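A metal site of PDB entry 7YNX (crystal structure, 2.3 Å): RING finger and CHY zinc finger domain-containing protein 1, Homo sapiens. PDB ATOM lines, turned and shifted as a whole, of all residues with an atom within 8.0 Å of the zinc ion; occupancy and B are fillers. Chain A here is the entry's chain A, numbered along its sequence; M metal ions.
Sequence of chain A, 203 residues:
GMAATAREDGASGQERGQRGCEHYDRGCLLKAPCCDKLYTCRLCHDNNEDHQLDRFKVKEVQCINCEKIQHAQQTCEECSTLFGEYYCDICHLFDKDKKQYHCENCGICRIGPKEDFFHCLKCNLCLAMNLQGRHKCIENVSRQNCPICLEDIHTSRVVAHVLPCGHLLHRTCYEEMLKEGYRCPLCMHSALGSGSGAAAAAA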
ATOM      1  N   GLY A  20      19.240 -32.087   1.103  1.00  0.00           N
ATOM      2  CA  GLY A  20      17.996 -31.425   0.776  1.00  0.00           C
ATOM      3  C   GLY A  20      17.024 -31.440   1.944  1.00  0.00           C
ATOM      4  O   GLY A  20      17.437 -31.399   3.104  1.00  0.00           O
ATOM      5  N   CYS A  21      15.729 -31.515   1.631  1.00  0.00           N
ATOM      6  CA  CYS A  21      14.681 -31.515   2.652  1.00  0.00           C
ATOM      7  C   CYS A  21      13.675 -32.622   2.369  1.00  0.00           C
ATOM      8  O   CYS A  21      13.924 -33.510   1.540  1.00  0.00           O
ATOM      9  CB  CYS A  21      13.966 -30.167   2.684  1.00  0.00           C
ATOM     10  SG  CYS A  21      13.304 -29.698   1.083  1.00  0.00           S
ATOM     11  N   GLU A  22      12.531 -32.569   3.057  1.00  0.00           N
ATOM     12  CA  GLU A  22      11.446 -33.517   2.813  1.00  0.00           C
ATOM     13  C   GLU A  22      10.824 -33.322   1.445  1.00  0.00           C
ATOM     14  O   GLU A  22      10.210 -34.260   0.915  1.00  0.00           O
ATOM     15  CB  GLU A  22      10.368 -33.381   3.893  1.00  0.00           C
ATOM     16  CG  GLU A  22       9.874 -31.952   4.111  1.00  0.00           C
ATOM     17  CD  GLU A  22       8.600 -31.874   4.937  1.00  0.00           C
ATOM     18  OE1 GLU A  22       8.257 -30.756   5.385  1.00  0.00           O
ATOM     19  OE2 GLU A  22       7.935 -32.923   5.116  1.00  0.00           O
ATOM     20  N   HIS A  23      10.949 -32.132   0.856  1.00  0.00           N
ATOM     21  CA  HIS A  23      10.327 -31.854  -0.431  1.00  0.00           C
ATOM     22  C   HIS A  23      11.267 -32.042  -1.600  1.00  0.00           C
ATOM     23  O   HIS A  23      10.809 -32.343  -2.715  1.00  0.00           O
ATOM     24  CB  HIS A  23       9.808 -30.423  -0.486  1.00  0.00           C
ATOM     25  CG  HIS A  23       9.127 -29.984   0.754  1.00  0.00           C
ATOM     26  ND1 HIS A  23       9.735 -29.206   1.707  1.00  0.00           N
ATOM     27  CD2 HIS A  23       7.869 -30.216   1.210  1.00  0.00           C
ATOM     28  CE1 HIS A  23       8.882 -28.950   2.689  1.00  0.00           C
ATOM     29  NE2 HIS A  23       7.746 -29.552   2.407  1.00  0.00           N
ATOM     30  N   TYR A  24      12.574 -31.845  -1.395  1.00  0.00           N
ATOM     31  CA  TYR A  24      13.498 -31.733  -2.505  1.00  0.00           C
ATOM     32  C   TYR A  24      14.812 -32.413  -2.181  1.00  0.00           C
ATOM     33  O   TYR A  24      15.258 -32.461  -1.022  1.00  0.00           O
ATOM     34  CB  TYR A  24      13.755 -30.248  -2.870  1.00  0.00           C
ATOM     35  CG  TYR A  24      12.556 -29.657  -3.542  1.00  0.00           C
ATOM     36  CD1 TYR A  24      12.271 -29.949  -4.872  1.00  0.00           C
ATOM     37  CD2 TYR A  24      11.665 -28.836  -2.844  1.00  0.00           C
ATOM     38  CE1 TYR A  24      11.156 -29.445  -5.497  1.00  0.00           C
ATOM     39  CE2 TYR A  24      10.546 -28.323  -3.465  1.00  0.00           C
ATOM     40  CZ  TYR A  24      10.297 -28.626  -4.791  1.00  0.00           C
ATOM     41  OH  TYR A  24       9.185 -28.128  -5.429  1.00  0.00           O
ATOM     42  N   ARG A  26      18.270 -31.495  -3.095  1.00  0.00           N
ATOM     43  CA  ARG A  26      18.970 -30.338  -3.654  1.00  0.00           C
ATOM     44  C   ARG A  26      20.224 -30.009  -2.850  1.00  0.00           C
ATOM     45  O   ARG A  26      20.296 -30.261  -1.638  1.00  0.00           O
ATOM     46  CB  ARG A  26      18.072 -29.092  -3.745  1.00  0.00           C
ATOM     47  CG  ARG A  26      17.579 -28.531  -2.430  1.00  0.00           C
ATOM     48  CD  ARG A  26      16.841 -27.192  -2.643  1.00  0.00           C
ATOM     49  NE  ARG A  26      15.717 -27.313  -3.571  1.00  0.00           N
ATOM     50  CZ  ARG A  26      14.842 -26.353  -3.844  1.00  0.00           C
ATOM     51  NH1 ARG A  26      14.943 -25.149  -3.271  1.00  0.00           N
ATOM     52  NH2 ARG A  26      13.852 -26.585  -4.705  1.00  0.00           N
ATOM     53  N   TYR A  39      16.396 -21.140   3.973  1.00  0.00           N
ATOM     54  CA  TYR A  39      15.515 -22.293   4.033  1.00  0.00           C
ATOM     55  C   TYR A  39      15.861 -23.219   2.885  1.00  0.00           C
ATOM     56  O   TYR A  39      16.267 -22.768   1.801  1.00  0.00           O
ATOM     57  CB  TYR A  39      14.019 -21.887   3.930  1.00  0.00           C
ATOM     58  CG  TYR A  39      13.445 -21.308   5.206  1.00  0.00           C
ATOM     59  CD1 TYR A  39      13.030 -22.142   6.248  1.00  0.00           C
ATOM     60  CD2 TYR A  39      13.302 -19.932   5.372  1.00  0.00           C
ATOM     61  CE1 TYR A  39      12.503 -21.625   7.403  1.00  0.00           C
ATOM     62  CE2 TYR A  39      12.782 -19.405   6.540  1.00  0.00           C
ATOM     63  CZ  TYR A  39      12.384 -20.253   7.544  1.00  0.00           C
ATOM     64  OH  TYR A  39      11.868 -19.736   8.709  1.00  0.00           O
ATOM     65  N   THR A  40      15.702 -24.525   3.110  1.00  0.00           N
ATOM     66  CA  THR A  40      16.048 -25.460   2.045  1.00  0.00           C
ATOM     67  C   THR A  40      15.217 -25.194   0.795  1.00  0.00           C
ATOM     68  O   THR A  40      15.754 -25.244  -0.332  1.00  0.00           O
ATOM     69  CB  THR A  40      15.860 -26.904   2.491  1.00  0.00           C
ATOM     70  OG1 THR A  40      16.480 -27.118   3.758  1.00  0.00           O
ATOM     71  CG2 THR A  40      16.500 -27.802   1.474  1.00  0.00           C
ATOM     72  N   CYS A  41      13.928 -24.909   0.950  1.00  0.00           N
ATOM     73  CA  CYS A  41      13.071 -24.668  -0.200  1.00  0.00           C
ATOM     74  C   CYS A  41      11.884 -23.803   0.203  1.00  0.00           C
ATOM     75  O   CYS A  41      11.649 -23.533   1.374  1.00  0.00           O
ATOM     76  CB  CYS A  41      12.597 -25.984  -0.816  1.00  0.00           C
ATOM     77  SG  CYS A  41      11.071 -26.640  -0.063  1.00  0.00           S
ATOM     78  N   ARG A  42      11.125 -23.373  -0.809  1.00  0.00           N
ATOM     79  CA  ARG A  42      10.033 -22.438  -0.561  1.00  0.00           C
ATOM     80  C   ARG A  42       8.976 -23.020   0.373  1.00  0.00           C
ATOM     81  O   ARG A  42       8.418 -22.308   1.215  1.00  0.00           O
ATOM     82  CB  ARG A  42       9.422 -21.980  -1.895  1.00  0.00           C
ATOM     83  CG  ARG A  42       8.460 -22.975  -2.559  1.00  0.00           C
ATOM     84  CD  ARG A  42       8.241 -22.592  -4.029  1.00  0.00           C
ATOM     85  NE  ARG A  42       7.344 -23.530  -4.722  1.00  0.00           N
ATOM     86  CZ  ARG A  42       7.736 -24.690  -5.221  1.00  0.00           C
ATOM     87  NH1 ARG A  42       9.005 -25.084  -5.104  1.00  0.00           N
ATOM     88  NH2 ARG A  42       6.845 -25.471  -5.842  1.00  0.00           N
ATOM     89  N   LEU A  43       8.702 -24.337   0.267  1.00  0.00           N
ATOM     90  CA  LEU A  43       7.760 -24.971   1.183  1.00  0.00           C
ATOM     91  C   LEU A  43       8.293 -24.986   2.619  1.00  0.00           C
ATOM     92  O   LEU A  43       7.543 -24.689   3.563  1.00  0.00           O
ATOM     93  CB  LEU A  43       7.458 -26.391   0.716  1.00  0.00           C
ATOM     94  CG  LEU A  43       7.041 -26.457  -0.748  1.00  0.00           C
ATOM     95  CD1 LEU A  43       6.637 -27.868  -1.096  1.00  0.00           C
ATOM     96  CD2 LEU A  43       5.916 -25.480  -1.044  1.00  0.00           C
ATOM     97  N   CYS A  44       9.574 -25.330   2.794  1.00  0.00           N
ATOM     98  CA  CYS A  44      10.182 -25.253   4.117  1.00  0.00           C
ATOM     99  C   CYS A  44      10.052 -23.853   4.692  1.00  0.00           C
ATOM    100  O   CYS A  44       9.888 -23.663   5.904  1.00  0.00           O
ATOM    101  CB  CYS A  44      11.655 -25.638   4.048  1.00  0.00           C
ATOM    102  SG  CYS A  44      11.950 -27.419   4.123  1.00  0.00           S
ATOM    103  N   HIS A  45      10.147 -22.852   3.821  1.00  0.00           N
ATOM    104  CA  HIS A  45      10.037 -21.471   4.282  1.00  0.00           C
ATOM    105  C   HIS A  45       8.589 -21.144   4.625  1.00  0.00           C
ATOM    106  O   HIS A  45       8.318 -20.532   5.660  1.00  0.00           O
ATOM    107  CB  HIS A  45      10.564 -20.535   3.200  1.00  0.00           C
ATOM    108  CG  HIS A  45      10.112 -19.126   3.332  1.00  0.00           C
ATOM    109  ND1 HIS A  45       8.796 -18.746   3.205  1.00  0.00           N
ATOM    110  CD2 HIS A  45      10.812 -17.996   3.579  1.00  0.00           C
ATOM    111  CE1 HIS A  45       8.700 -17.443   3.374  1.00  0.00           C
ATOM    112  NE2 HIS A  45       9.905 -16.967   3.608  1.00  0.00           N
ATOM    113  N   ASP A  46       7.663 -21.551   3.752  1.00  0.00           N
ATOM    114  CA  ASP A  46       6.265 -21.174   3.917  1.00  0.00           C
ATOM    115  C   ASP A  46       5.630 -21.881   5.097  1.00  0.00           C
ATOM    116  O   ASP A  46       4.740 -21.322   5.740  1.00  0.00           O
ATOM    117  CB  ASP A  46       5.501 -21.470   2.632  1.00  0.00           C
ATOM    118  CG  ASP A  46       5.892 -20.532   1.500  1.00  0.00           C
ATOM    119  OD1 ASP A  46       6.536 -19.483   1.756  1.00  0.00           O
ATOM    120  OD2 ASP A  46       5.545 -20.843   0.339  1.00  0.00           O
ATOM    121  N   ASN A  47       6.104 -23.089   5.421  1.00  0.00           N
ATOM    122  CA  ASN A  47       5.660 -23.768   6.624  1.00  0.00           C
ATOM    123  C   ASN A  47       6.184 -23.132   7.908  1.00  0.00           C
ATOM    124  O   ASN A  47       5.767 -23.554   8.993  1.00  0.00           O
ATOM    125  CB  ASN A  47       6.101 -25.239   6.588  1.00  0.00           C
ATOM    126  CG  ASN A  47       5.430 -26.038   5.475  1.00  0.00           C
ATOM    127  OD1 ASN A  47       4.613 -25.522   4.720  1.00  0.00           O
ATOM    128  ND2 ASN A  47       5.793 -27.318   5.362  1.00  0.00           N
ATOM    129  N   ASN A  48       7.096 -22.153   7.830  1.00  0.00           N
ATOM    130  CA  ASN A  48       7.707 -21.605   9.045  1.00  0.00           C
ATOM    131  C   ASN A  48       7.729 -20.090   9.062  1.00  0.00           C
ATOM    132  O   ASN A  48       8.508 -19.503   9.818  1.00  0.00           O
ATOM    133  CB  ASN A  48       9.138 -22.130   9.219  1.00  0.00           C
ATOM    134  CG  ASN A  48       9.179 -23.628   9.403  1.00  0.00           C
ATOM    135  OD1 ASN A  48       8.755 -24.146  10.435  1.00  0.00           O
ATOM    136  ND2 ASN A  48       9.665 -24.337   8.389  1.00  0.00           N
ATOM    137  N   ARG A 157       1.501 -29.166  -5.705  1.00  0.00           N
ATOM    138  CA  ARG A 157       2.284 -30.323  -6.156  1.00  0.00           C
ATOM    139  C   ARG A 157       1.454 -31.603  -6.250  1.00  0.00           C
ATOM    140  O   ARG A 157       1.984 -32.651  -6.640  1.00  0.00           O
ATOM    141  CB  ARG A 157       3.504 -30.549  -5.258  1.00  0.00           C
ATOM    142  CG  ARG A 157       4.479 -29.397  -5.253  1.00  0.00           C
ATOM    143  CD  ARG A 157       5.785 -29.788  -4.556  1.00  0.00           C
ATOM    144  NE  ARG A 157       5.514 -30.334  -3.230  1.00  0.00           N
ATOM    145  CZ  ARG A 157       6.365 -31.113  -2.556  1.00  0.00           C
ATOM    146  NH1 ARG A 157       7.540 -31.436  -3.094  1.00  0.00           N
ATOM    147  NH2 ARG A 157       6.019 -31.564  -1.350  1.00  0.00           N
HETATM  148 ZN    ZN M   1      11.505 -28.116   1.890  1.00  0.00          ZN
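The backbone NH (N) of Tyr 24 sits close to the side-chain sulfur (SG) of Cys 21. The backbone carbonyl oxygen of His 23 lies within hydrogen-bond range of the guanidinium group of Arg 157. The backbone carbonyl oxygen of Cys 44 is in hydrogen-bond range of the side-chain amide nitrogen of Asn 48 (2.6 Å). The side-chain carboxylate (OE1) of Glu 22 sits at hydrogen-bond distance from a ring nitrogen (NE2) of His 23, 3.3 Å away. The backbone NH (N) of Leu 43 sits close to the side-chain sulfur (SG) of Cys 41 (3.3 Å).
Of the 17 residues printed, 4 come within 4 Å of the zinc ion. The nearest printed residue that does not touch the zinc ion is Leu 43 (4.5 Å).
The zinc ion is bound by ND1 of His 23 (2.1 Å), SG of Cys 44 (2.4 Å), SG of Cys 41 (2.5 Å) and SG of Cys 21 (2.5 Å). The zinc ion has four donor atoms within binding distance.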
